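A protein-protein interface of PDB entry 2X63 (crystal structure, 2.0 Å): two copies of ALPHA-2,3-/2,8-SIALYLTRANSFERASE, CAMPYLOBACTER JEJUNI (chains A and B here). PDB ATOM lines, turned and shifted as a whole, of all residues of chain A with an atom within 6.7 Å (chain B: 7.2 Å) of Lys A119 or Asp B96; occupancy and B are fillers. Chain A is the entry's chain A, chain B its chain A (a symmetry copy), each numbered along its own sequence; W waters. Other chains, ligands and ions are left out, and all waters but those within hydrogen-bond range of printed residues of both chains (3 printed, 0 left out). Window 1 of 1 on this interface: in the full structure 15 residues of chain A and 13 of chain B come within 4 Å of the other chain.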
ATOM      1  N   TYR A  80       2.815  20.273  -3.452  1.00  0.00           N
ATOM      2  CA  TYR A  80       2.504  20.759  -2.108  1.00  0.00           C
ATOM      3  C   TYR A  80       3.014  22.179  -1.856  1.00  0.00           C
ATOM      4  O   TYR A  80       2.826  22.714  -0.764  1.00  0.00           O
ATOM      5  CB  TYR A  80       3.146  19.848  -1.069  1.00  0.00           C
ATOM      6  CG  TYR A  80       2.537  18.463  -0.913  1.00  0.00           C
ATOM      7  CD1 TYR A  80       3.152  17.341  -1.460  1.00  0.00           C
ATOM      8  CD2 TYR A  80       1.365  18.277  -0.192  1.00  0.00           C
ATOM      9  CE1 TYR A  80       2.610  16.071  -1.281  1.00  0.00           C
ATOM     10  CE2 TYR A  80       0.822  17.021  -0.010  1.00  0.00           C
ATOM     11  CZ  TYR A  80       1.444  15.927  -0.551  1.00  0.00           C
ATOM     12  OH  TYR A  80       0.883  14.687  -0.368  1.00  0.00           O
ATOM     13  N   ASN A  81       3.662  22.776  -2.850  1.00  0.00           N
ATOM     14  CA  ASN A  81       4.373  24.042  -2.654  1.00  0.00           C
ATOM     15  C   ASN A  81       5.396  23.931  -1.499  1.00  0.00           C
ATOM     16  O   ASN A  81       5.399  24.724  -0.550  1.00  0.00           O
ATOM     17  CB  ASN A  81       3.397  25.214  -2.446  1.00  0.00           C
ATOM     18  CG  ASN A  81       2.877  25.784  -3.766  1.00  0.00           C
ATOM     19  OD1 ASN A  81       2.908  25.117  -4.795  1.00  0.00           O
ATOM     20  ND2 ASN A  81       2.419  27.040  -3.739  1.00  0.00           N
ATOM     21  N   GLN A  82       6.256  22.922  -1.595  1.00  0.00           N
ATOM     22  CA  GLN A  82       7.349  22.738  -0.642  1.00  0.00           C
ATOM     23  C   GLN A  82       8.639  22.574  -1.447  1.00  0.00           C
ATOM     24  O   GLN A  82       8.720  21.706  -2.315  1.00  0.00           O
ATOM     25  CB  GLN A  82       7.110  21.485   0.204  1.00  0.00           C
ATOM     26  CG  GLN A  82       5.911  21.547   1.141  1.00  0.00           C
ATOM     27  CD  GLN A  82       6.163  22.425   2.341  1.00  0.00           C
ATOM     28  OE1 GLN A  82       5.856  23.629   2.336  1.00  0.00           O
ATOM     29  NE2 GLN A  82       6.741  21.842   3.375  1.00  0.00           N
ATOM     30  N   LEU A  85      10.065  19.125  -1.777  1.00  0.00           N
ATOM     31  CA  LEU A  85       9.252  18.093  -2.424  1.00  0.00           C
ATOM     32  C   LEU A  85       9.136  18.254  -3.930  1.00  0.00           C
ATOM     33  O   LEU A  85       8.701  17.335  -4.621  1.00  0.00           O
ATOM     34  CB  LEU A  85       7.839  18.036  -1.821  1.00  0.00           C
ATOM     35  CG  LEU A  85       7.796  17.652  -0.339  1.00  0.00           C
ATOM     36  CD1 LEU A  85       6.363  17.648   0.176  1.00  0.00           C
ATOM     37  CD2 LEU A  85       8.465  16.289  -0.102  1.00  0.00           C
ATOM     38  N   TYR A 105      -2.144  20.951  -6.019  1.00  0.00           N
ATOM     39  CA  TYR A 105      -2.174  21.879  -4.896  1.00  0.00           C
ATOM     40  C   TYR A 105      -3.213  22.987  -5.085  1.00  0.00           C
ATOM     41  O   TYR A 105      -3.646  23.577  -4.114  1.00  0.00           O
ATOM     42  CB  TYR A 105      -0.808  22.519  -4.709  1.00  0.00           C
ATOM     43  CG  TYR A 105      -0.614  23.218  -3.373  1.00  0.00           C
ATOM     44  CD1 TYR A 105      -0.326  24.576  -3.313  1.00  0.00           C
ATOM     45  CD2 TYR A 105      -0.688  22.513  -2.181  1.00  0.00           C
ATOM     46  CE1 TYR A 105      -0.121  25.216  -2.098  1.00  0.00           C
ATOM     47  CE2 TYR A 105      -0.484  23.143  -0.966  1.00  0.00           C
ATOM     48  CZ  TYR A 105      -0.195  24.490  -0.938  1.00  0.00           C
ATOM     49  OH  TYR A 105       0.023  25.116   0.266  1.00  0.00           O
ATOM     50  N   PHE A 108      -5.847  21.017  -3.314  1.00  0.00           N
ATOM     51  CA  PHE A 108      -5.429  20.617  -1.973  1.00  0.00           C
ATOM     52  C   PHE A 108      -5.444  21.816  -1.025  1.00  0.00           C
ATOM     53  O   PHE A 108      -5.926  21.715   0.088  1.00  0.00           O
ATOM     54  CB  PHE A 108      -4.015  20.025  -2.065  1.00  0.00           C
ATOM     55  CG  PHE A 108      -3.480  19.447  -0.775  1.00  0.00           C
ATOM     56  CD1 PHE A 108      -2.750  20.235   0.105  1.00  0.00           C
ATOM     57  CD2 PHE A 108      -3.643  18.091  -0.481  1.00  0.00           C
ATOM     58  CE1 PHE A 108      -2.223  19.702   1.267  1.00  0.00           C
ATOM     59  CE2 PHE A 108      -3.129  17.555   0.678  1.00  0.00           C
ATOM     60  CZ  PHE A 108      -2.413  18.363   1.564  1.00  0.00           C
ATOM     61  N   LYS A 109      -4.910  22.955  -1.460  1.00  0.00           N
ATOM     62  CA  LYS A 109      -4.830  24.112  -0.577  1.00  0.00           C
ATOM     63  C   LYS A 109      -6.194  24.717  -0.244  1.00  0.00           C
ATOM     64  O   LYS A 109      -6.309  25.516   0.683  1.00  0.00           O
ATOM     65  CB  LYS A 109      -3.890  25.177  -1.161  1.00  0.00           C
ATOM     66  CG  LYS A 109      -4.460  25.967  -2.331  1.00  0.00           C
ATOM     67  CD  LYS A 109      -3.397  26.880  -2.959  1.00  0.00           C
ATOM     68  CE  LYS A 109      -4.026  27.752  -4.042  1.00  0.00           C
ATOM     69  NZ  LYS A 109      -3.019  28.307  -4.989  1.00  0.00           N
ATOM     70  N   PHE A 114      -6.725  20.797   6.387  1.00  0.00           N
ATOM     71  CA  PHE A 114      -5.914  19.640   6.010  1.00  0.00           C
ATOM     72  C   PHE A 114      -4.537  20.038   5.486  1.00  0.00           C
ATOM     73  O   PHE A 114      -3.550  19.353   5.751  1.00  0.00           O
ATOM     74  CB  PHE A 114      -6.618  18.722   5.010  1.00  0.00           C
ATOM     75  CG  PHE A 114      -5.913  17.406   4.824  1.00  0.00           C
ATOM     76  CD1 PHE A 114      -5.833  16.496   5.874  1.00  0.00           C
ATOM     77  CD2 PHE A 114      -5.309  17.085   3.618  1.00  0.00           C
ATOM     78  CE1 PHE A 114      -5.175  15.293   5.726  1.00  0.00           C
ATOM     79  CE2 PHE A 114      -4.654  15.873   3.463  1.00  0.00           C
ATOM     80  CZ  PHE A 114      -4.596  14.973   4.518  1.00  0.00           C
ATOM     81  N   ASN A 115      -4.472  21.132   4.729  1.00  0.00           N
ATOM     82  CA  ASN A 115      -3.171  21.668   4.330  1.00  0.00           C
ATOM     83  C   ASN A 115      -2.332  21.868   5.603  1.00  0.00           C
ATOM     84  O   ASN A 115      -1.207  21.387   5.693  1.00  0.00           O
ATOM     85  CB  ASN A 115      -3.341  22.978   3.536  1.00  0.00           C
ATOM     86  CG  ASN A 115      -2.092  23.362   2.744  1.00  0.00           C
ATOM     87  OD1 ASN A 115      -1.113  22.606   2.672  1.00  0.00           O
ATOM     88  ND2 ASN A 115      -2.119  24.548   2.150  1.00  0.00           N
ATOM     89  N   ALA A 116      -2.888  22.543   6.605  1.00  0.00           N
ATOM     90  CA  ALA A 116      -2.145  22.783   7.846  1.00  0.00           C
ATOM     91  C   ALA A 116      -1.734  21.476   8.551  1.00  0.00           C
ATOM     92  O   ALA A 116      -0.609  21.344   9.072  1.00  0.00           O
ATOM     93  CB  ALA A 116      -2.955  23.674   8.797  1.00  0.00           C
ATOM     94  N   TYR A 117      -2.660  20.527   8.580  1.00  0.00           N
ATOM     95  CA  TYR A 117      -2.414  19.221   9.176  1.00  0.00           C
ATOM     96  C   TYR A 117      -1.225  18.542   8.491  1.00  0.00           C
ATOM     97  O   TYR A 117      -0.297  18.089   9.157  1.00  0.00           O
ATOM     98  CB  TYR A 117      -3.678  18.368   9.051  1.00  0.00           C
ATOM     99  CG  TYR A 117      -3.572  16.961   9.608  1.00  0.00           C
ATOM    100  CD1 TYR A 117      -2.923  15.962   8.897  1.00  0.00           C
ATOM    101  CD2 TYR A 117      -4.161  16.628  10.825  1.00  0.00           C
ATOM    102  CE1 TYR A 117      -2.838  14.672   9.389  1.00  0.00           C
ATOM    103  CE2 TYR A 117      -4.083  15.339  11.324  1.00  0.00           C
ATOM    104  CZ  TYR A 117      -3.414  14.370  10.598  1.00  0.00           C
ATOM    105  OH  TYR A 117      -3.324  13.093  11.084  1.00  0.00           O
ATOM    106  N   PHE A 118      -1.258  18.490   7.160  1.00  0.00           N
ATOM    107  CA  PHE A 118      -0.201  17.868   6.380  1.00  0.00           C
ATOM    108  C   PHE A 118       1.150  18.517   6.614  1.00  0.00           C
ATOM    109  O   PHE A 118       2.142  17.840   6.892  1.00  0.00           O
ATOM    110  CB  PHE A 118      -0.500  17.942   4.874  1.00  0.00           C
ATOM    111  CG  PHE A 118       0.694  17.587   4.030  1.00  0.00           C
ATOM    112  CD1 PHE A 118       0.983  16.265   3.735  1.00  0.00           C
ATOM    113  CD2 PHE A 118       1.569  18.568   3.587  1.00  0.00           C
ATOM    114  CE1 PHE A 118       2.109  15.928   2.991  1.00  0.00           C
ATOM    115  CE2 PHE A 118       2.697  18.226   2.840  1.00  0.00           C
ATOM    116  CZ  PHE A 118       2.963  16.907   2.548  1.00  0.00           C
ATOM    117  N   LYS A 119       1.201  19.838   6.459  1.00  0.00           N
ATOM    118  CA  LYS A 119       2.473  20.563   6.549  1.00  0.00           C
ATOM    119  C   LYS A 119       3.138  20.383   7.904  1.00  0.00           C
ATOM    120  O   LYS A 119       4.345  20.139   7.989  1.00  0.00           O
ATOM    121  CB  LYS A 119       2.263  22.060   6.263  1.00  0.00           C
ATOM    122  CG  LYS A 119       1.845  22.363   4.817  1.00  0.00           C
ATOM    123  CD  LYS A 119       2.980  22.065   3.821  1.00  0.00           C
ATOM    124  CE  LYS A 119       2.447  21.932   2.398  1.00  0.00           C
ATOM    125  NZ  LYS A 119       1.730  23.193   1.917  1.00  0.00           N
ATOM    126  N   PHE A 120       2.356  20.499   8.971  1.00  0.00           N
ATOM    127  CA  PHE A 120       2.913  20.357  10.320  1.00  0.00           C
ATOM    128  C   PHE A 120       3.545  18.974  10.527  1.00  0.00           C
ATOM    129  O   PHE A 120       4.699  18.867  10.968  1.00  0.00           O
ATOM    130  CB  PHE A 120       1.855  20.631  11.398  1.00  0.00           C
ATOM    131  CG  PHE A 120       2.357  20.422  12.799  1.00  0.00           C
ATOM    132  CD1 PHE A 120       3.228  21.333  13.379  1.00  0.00           C
ATOM    133  CD2 PHE A 120       1.970  19.311  13.534  1.00  0.00           C
ATOM    134  CE1 PHE A 120       3.706  21.138  14.685  1.00  0.00           C
ATOM    135  CE2 PHE A 120       2.444  19.117  14.837  1.00  0.00           C
ATOM    136  CZ  PHE A 120       3.310  20.028  15.406  1.00  0.00           C
ATOM    137  N   HIS A 121       2.791  17.923  10.200  1.00  0.00           N
ATOM    138  CA  HIS A 121       3.302  16.554  10.297  1.00  0.00           C
ATOM    139  C   HIS A 121       4.505  16.313   9.374  1.00  0.00           C
ATOM    140  O   HIS A 121       5.475  15.678   9.769  1.00  0.00           O
ATOM    141  CB  HIS A 121       2.193  15.527   9.995  1.00  0.00           C
ATOM    142  CG  HIS A 121       1.104  15.501  11.022  1.00  0.00           C
ATOM    143  ND1 HIS A 121       0.069  16.409  11.030  1.00  0.00           N
ATOM    144  CD2 HIS A 121       0.897  14.685  12.083  1.00  0.00           C
ATOM    145  CE1 HIS A 121      -0.725  16.162  12.057  1.00  0.00           C
ATOM    146  NE2 HIS A 121      -0.253  15.115  12.707  1.00  0.00           N
ATOM    147  N   GLU A 122       4.435  16.797   8.139  1.00  0.00           N
ATOM    148  CA  GLU A 122       5.553  16.610   7.201  1.00  0.00           C
ATOM    149  C   GLU A 122       6.824  17.354   7.665  1.00  0.00           C
ATOM    150  O   GLU A 122       7.907  16.769   7.805  1.00  0.00           O
ATOM    151  CB  GLU A 122       5.165  17.072   5.793  1.00  0.00           C
ATOM    152  CG  GLU A 122       6.370  17.313   4.875  1.00  0.00           C
ATOM    153  CD  GLU A 122       7.187  16.052   4.670  1.00  0.00           C
ATOM    154  OE1 GLU A 122       6.585  14.954   4.751  1.00  0.00           O
ATOM    155  OE2 GLU A 122       8.419  16.150   4.435  1.00  0.00           O
ATOM    156  N   ILE A 123       6.687  18.653   7.885  1.00  0.00           N
ATOM    157  CA  ILE A 123       7.841  19.492   8.207  1.00  0.00           C
ATOM    158  C   ILE A 123       8.488  19.148   9.544  1.00  0.00           C
ATOM    159  O   ILE A 123       9.716  19.015   9.640  1.00  0.00           O
ATOM    160  CB  ILE A 123       7.461  20.992   8.231  1.00  0.00           C
ATOM    161  CG1 ILE A 123       7.102  21.478   6.819  1.00  0.00           C
ATOM    162  CG2 ILE A 123       8.611  21.818   8.830  1.00  0.00           C
ATOM    163  CD1 ILE A 123       6.245  22.744   6.800  1.00  0.00           C
ATOM    164  N   TYR A 124       7.670  19.002  10.580  1.00  0.00           N
ATOM    165  CA  TYR A 124       8.212  18.898  11.927  1.00  0.00           C
ATOM    166  C   TYR A 124       8.397  17.456  12.402  1.00  0.00           C
ATOM    167  O   TYR A 124       9.294  17.175  13.195  1.00  0.00           O
ATOM    168  CB  TYR A 124       7.347  19.667  12.914  1.00  0.00           C
ATOM    169  CG  TYR A 124       7.372  21.173  12.733  1.00  0.00           C
ATOM    170  CD1 TYR A 124       6.344  21.831  12.062  1.00  0.00           C
ATOM    171  CD2 TYR A 124       8.410  21.939  13.261  1.00  0.00           C
ATOM    172  CE1 TYR A 124       6.351  23.207  11.907  1.00  0.00           C
ATOM    173  CE2 TYR A 124       8.426  23.332  13.109  1.00  0.00           C
ATOM    174  CZ  TYR A 124       7.395  23.958  12.442  1.00  0.00           C
ATOM    175  OH  TYR A 124       7.412  25.337  12.287  1.00  0.00           O
ATOM    176  N   PHE A 125       7.561  16.547  11.905  1.00  0.00           N
ATOM    177  CA  PHE A 125       7.637  15.154  12.350  1.00  0.00           C
ATOM    178  C   PHE A 125       8.006  14.170  11.247  1.00  0.00           C
ATOM    179  O   PHE A 125       8.106  12.974  11.498  1.00  0.00           O
ATOM    180  CB  PHE A 125       6.325  14.739  13.005  1.00  0.00           C
ATOM    181  CG  PHE A 125       6.092  15.397  14.331  1.00  0.00           C
ATOM    182  CD1 PHE A 125       5.367  16.570  14.420  1.00  0.00           C
ATOM    183  CD2 PHE A 125       6.638  14.871  15.483  1.00  0.00           C
ATOM    184  CE1 PHE A 125       5.173  17.194  15.639  1.00  0.00           C
ATOM    185  CE2 PHE A 125       6.437  15.491  16.712  1.00  0.00           C
ATOM    186  CZ  PHE A 125       5.698  16.658  16.778  1.00  0.00           C
ATOM    187  N   GLN A 127       6.275  13.014   8.967  1.00  0.00           N
ATOM    188  CA  GLN A 127       5.181  12.076   8.773  1.00  0.00           C
ATOM    189  C   GLN A 127       4.421  12.516   7.517  1.00  0.00           C
ATOM    190  O   GLN A 127       3.755  13.555   7.499  1.00  0.00           O
ATOM    191  CB  GLN A 127       4.292  12.005  10.027  1.00  0.00           C
ATOM    192  CG  GLN A 127       5.023  11.414  11.233  1.00  0.00           C
ATOM    193  CD  GLN A 127       4.273  11.550  12.542  1.00  0.00           C
ATOM    194  OE1 GLN A 127       4.726  11.055  13.573  1.00  0.00           O
ATOM    195  NE2 GLN A 127       3.135  12.225  12.519  1.00  0.00           N
ATOM    196  N   TYR B  58       6.102  28.407  16.255  1.00  0.00           N
ATOM    197  CA  TYR B  58       4.944  27.738  15.668  1.00  0.00           C
ATOM    198  C   TYR B  58       4.906  26.300  16.158  1.00  0.00           C
ATOM    199  O   TYR B  58       3.883  25.823  16.635  1.00  0.00           O
ATOM    200  CB  TYR B  58       4.987  27.806  14.129  1.00  0.00           C
ATOM    201  CG  TYR B  58       3.775  27.180  13.453  1.00  0.00           C
ATOM    202  CD1 TYR B  58       2.610  27.923  13.238  1.00  0.00           C
ATOM    203  CD2 TYR B  58       3.794  25.851  13.028  1.00  0.00           C
ATOM    204  CE1 TYR B  58       1.497  27.351  12.616  1.00  0.00           C
ATOM    205  CE2 TYR B  58       2.688  25.272  12.416  1.00  0.00           C
ATOM    206  CZ  TYR B  58       1.541  26.026  12.212  1.00  0.00           C
ATOM    207  OH  TYR B  58       0.447  25.456  11.603  1.00  0.00           O
ATOM    208  N   LYS B  92       7.624  35.052   1.438  1.00  0.00           N
ATOM    209  CA  LYS B  92       7.011  34.670   0.169  1.00  0.00           C
ATOM    210  C   LYS B  92       6.266  33.327   0.258  1.00  0.00           C
ATOM    211  O   LYS B  92       5.159  33.190  -0.248  1.00  0.00           O
ATOM    212  CB  LYS B  92       8.054  34.652  -0.946  1.00  0.00           C
ATOM    213  CG  LYS B  92       7.573  33.990  -2.237  1.00  0.00           C
ATOM    214  CD  LYS B  92       8.729  33.892  -3.241  1.00  0.00           C
ATOM    215  CE  LYS B  92       8.371  32.995  -4.429  1.00  0.00           C
ATOM    216  NZ  LYS B  92       9.404  33.122  -5.494  1.00  0.00           N
ATOM    217  N   THR B  93       6.860  32.345   0.925  1.00  0.00           N
ATOM    218  CA  THR B  93       6.272  31.003   1.023  1.00  0.00           C
ATOM    219  C   THR B  93       5.424  30.772   2.296  1.00  0.00           C
ATOM    220  O   THR B  93       4.986  29.653   2.559  1.00  0.00           O
ATOM    221  CB  THR B  93       7.385  29.951   1.025  1.00  0.00           C
ATOM    222  OG1 THR B  93       8.148  30.090   2.233  1.00  0.00           O
ATOM    223  CG2 THR B  93       8.314  30.124  -0.204  1.00  0.00           C
ATOM    224  N   PHE B  94       5.200  31.818   3.078  1.00  0.00           N
ATOM    225  CA  PHE B  94       4.607  31.679   4.410  1.00  0.00           C
ATOM    226  C   PHE B  94       3.339  30.831   4.452  1.00  0.00           C
ATOM    227  O   PHE B  94       3.221  29.935   5.278  1.00  0.00           O
ATOM    228  CB  PHE B  94       4.290  33.059   4.997  1.00  0.00           C
ATOM    229  CG  PHE B  94       3.768  33.021   6.412  1.00  0.00           C
ATOM    230  CD1 PHE B  94       4.643  32.956   7.486  1.00  0.00           C
ATOM    231  CD2 PHE B  94       2.403  33.075   6.669  1.00  0.00           C
ATOM    232  CE1 PHE B  94       4.169  32.945   8.798  1.00  0.00           C
ATOM    233  CE2 PHE B  94       1.921  33.065   7.984  1.00  0.00           C
ATOM    234  CZ  PHE B  94       2.803  32.997   9.042  1.00  0.00           C
ATOM    235  N   TYR B  95       2.368  31.151   3.600  1.00  0.00           N
ATOM    236  CA  TYR B  95       1.088  30.474   3.671  1.00  0.00           C
ATOM    237  C   TYR B  95       1.174  29.024   3.214  1.00  0.00           C
ATOM    238  O   TYR B  95       0.267  28.229   3.476  1.00  0.00           O
ATOM    239  CB  TYR B  95       0.005  31.253   2.907  1.00  0.00           C
ATOM    240  CG  TYR B  95      -0.403  32.511   3.633  1.00  0.00           C
ATOM    241  CD1 TYR B  95      -1.277  32.451   4.721  1.00  0.00           C
ATOM    242  CD2 TYR B  95       0.070  33.758   3.233  1.00  0.00           C
ATOM    243  CE1 TYR B  95      -1.666  33.606   5.401  1.00  0.00           C
ATOM    244  CE2 TYR B  95      -0.301  34.919   3.910  1.00  0.00           C
ATOM    245  CZ  TYR B  95      -1.167  34.833   5.001  1.00  0.00           C
ATOM    246  OH  TYR B  95      -1.546  35.973   5.672  1.00  0.00           O
ATOM    247  N   ASP B  96       2.282  28.665   2.576  1.00  0.00           N
ATOM    248  CA  ASP B  96       2.462  27.289   2.162  1.00  0.00           C
ATOM    249  C   ASP B  96       3.147  26.438   3.238  1.00  0.00           C
ATOM    250  O   ASP B  96       2.922  25.220   3.301  1.00  0.00           O
ATOM    251  CB  ASP B  96       3.174  27.224   0.803  1.00  0.00           C
ATOM    252  CG  ASP B  96       2.326  27.809  -0.312  1.00  0.00           C
ATOM    253  OD1 ASP B  96       1.098  27.545  -0.327  1.00  0.00           O
ATOM    254  OD2 ASP B  96       2.874  28.527  -1.165  1.00  0.00           O
ATOM    255  N   TYR B  97       3.968  27.074   4.085  1.00  0.00           N
ATOM    256  CA  TYR B  97       4.567  26.403   5.238  1.00  0.00           C
ATOM    257  C   TYR B  97       3.695  26.436   6.495  1.00  0.00           C
ATOM    258  O   TYR B  97       3.766  25.509   7.313  1.00  0.00           O
ATOM    259  CB  TYR B  97       5.985  26.938   5.532  1.00  0.00           C
ATOM    260  CG  TYR B  97       6.951  26.425   4.501  1.00  0.00           C
ATOM    261  CD1 TYR B  97       7.788  25.346   4.775  1.00  0.00           C
ATOM    262  CD2 TYR B  97       6.953  26.955   3.212  1.00  0.00           C
ATOM    263  CE1 TYR B  97       8.634  24.842   3.807  1.00  0.00           C
ATOM    264  CE2 TYR B  97       7.788  26.451   2.234  1.00  0.00           C
ATOM    265  CZ  TYR B  97       8.629  25.397   2.540  1.00  0.00           C
ATOM    266  OH  TYR B  97       9.450  24.905   1.571  1.00  0.00           O
ATOM    267  N   PHE B  98       2.869  27.478   6.629  1.00  0.00           N
ATOM    268  CA  PHE B  98       2.028  27.662   7.811  1.00  0.00           C
ATOM    269  C   PHE B  98       0.595  28.021   7.402  1.00  0.00           C
ATOM    270  O   PHE B  98       0.165  29.157   7.581  1.00  0.00           O
ATOM    271  CB  PHE B  98       2.614  28.754   8.716  1.00  0.00           C
ATOM    272  CG  PHE B  98       4.084  28.594   8.982  1.00  0.00           C
ATOM    273  CD1 PHE B  98       5.009  29.365   8.301  1.00  0.00           C
ATOM    274  CD2 PHE B  98       4.540  27.648   9.889  1.00  0.00           C
ATOM    275  CE1 PHE B  98       6.371  29.202   8.527  1.00  0.00           C
ATOM    276  CE2 PHE B  98       5.892  27.478  10.120  1.00  0.00           C
ATOM    277  CZ  PHE B  98       6.809  28.256   9.431  1.00  0.00           C
ATOM    278  N   PRO B  99      -0.153  27.049   6.854  1.00  0.00           N
ATOM    279  CA  PRO B  99      -1.416  27.414   6.194  1.00  0.00           C
ATOM    280  C   PRO B  99      -2.503  27.937   7.121  1.00  0.00           C
ATOM    281  O   PRO B  99      -3.469  28.536   6.639  1.00  0.00           O
ATOM    282  CB  PRO B  99      -1.864  26.104   5.516  1.00  0.00           C
ATOM    283  CG  PRO B  99      -0.590  25.312   5.356  1.00  0.00           C
ATOM    284  CD  PRO B  99       0.236  25.654   6.580  1.00  0.00           C
HETATM  285  O   HOH W   1       0.906  23.696   9.364  1.00  0.00           O
HETATM  286  O   HOH W   2      -1.891  27.901   2.228  1.00  0.00           O
HETATM  287  O   HOH W   3       3.695  23.438   9.520  1.00  0.00           O
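Among the printed residues, pairs that only touch across the chains: Gln A82 with Tyr B97 (3.3 Å), Asn A115 with Pro B99 (3.6 Å), Ala A116 with Pro B99 (3.8 Å), Lys A119 with Tyr B97 (3.9 Å), Lys A119 with Pro B99 (3.9 Å), Ile A123 with Tyr B97 (3.6 Å), Tyr A124 with Tyr B58 (3.7 Å) and Tyr A124 with Phe B98 (3.4 Å).
Lys A119 touches three residues of chain B. Of the printed residues of chain B, Asn A115 touches Pro B99 (3.6 Å). Printed residues of chain A within 4 Å of Phe B98: Tyr A124 (3.4 Å). Of the printed residues of chain B, Tyr A105 touches Asp B96 (2.7 Å). Of the printed residues of chain A, Tyr B97 touches Gln A82, Lys A119 and Ile A123. Of the printed residues of chain B, Gln A82 touches Asp B96 and Tyr B97. Tyr A80 touches none of the printed residues of chain B. The nearest residue of chain A that does not touch Asp B96 is Tyr A80 (4.8 Å).
The side-chain amide nitrogen (ND2) of Asn A81 is in hydrogen-bond range of the side-chain carboxylate (OD2) of Asp B96 (3.0 Å). The side-chain amino group (NZ) of Lys A119 sits at hydrogen-bond distance from the backbone carbonyl oxygen (O) of Asp B96 (2.7 Å). The side-chain hydroxyl (OH) of Tyr A105 lies within hydrogen-bond range of the side-chain carboxylate (OD1) of Asp B96. The side-chain amide oxygen of Gln A82 sits close to the backbone carbonyl oxygen of Asp B96, 3.5 Å away.
Water W2 lies within hydrogen-bond range of O of Tyr B95 (2.5 Å) and ND2 of Asn A115 (3.4 Å). Water W1 bridges the backbone carbonyl oxygen of Ala A116 (2.8 Å) and the side-chain hydroxyl of Tyr B58 (2.9 Å). Water W3 bridges the backbone carbonyl oxygen (O) of Tyr B97 (3.0 Å) and the backbone NH (N) of Phe A120 (3.3 Å).
The side-chain amide oxygen (OD1) of Asn A115 lies within hydrogen-bond range of the side-chain amino group (NZ) of Lys A119, at 3.0 Å. OH of Tyr A105 is in hydrogen-bond range of ND2 of Asn A115 (2.9 Å). The side-chain hydroxyl (OH) of Tyr A105 is in hydrogen-bond range of the side-chain amino group (NZ) of Lys A119, 3.1 Å away. O of Tyr A80 is in hydrogen-bond range of NZ of Lys A119 (2.9 Å).
Hydrophobic or aromatic side chains of chain A within 4 Å of the printed part of chain B: Tyr A105, Ile A123 and Tyr A124. Printed residues of chain B that touch a printed residue of chain A: Tyr B58, Asp B96, Tyr B97, Phe B98 and Pro B99. Among the printed residues, no Asp or Glu carboxylate lies within 4 Å of a Lys or Arg side-chain nitrogen of the other chain.
No position is printed for both chains. Of the 12 pairs that touch across the chains among the printed residues, none has its exchanged pair printed and touching as well.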
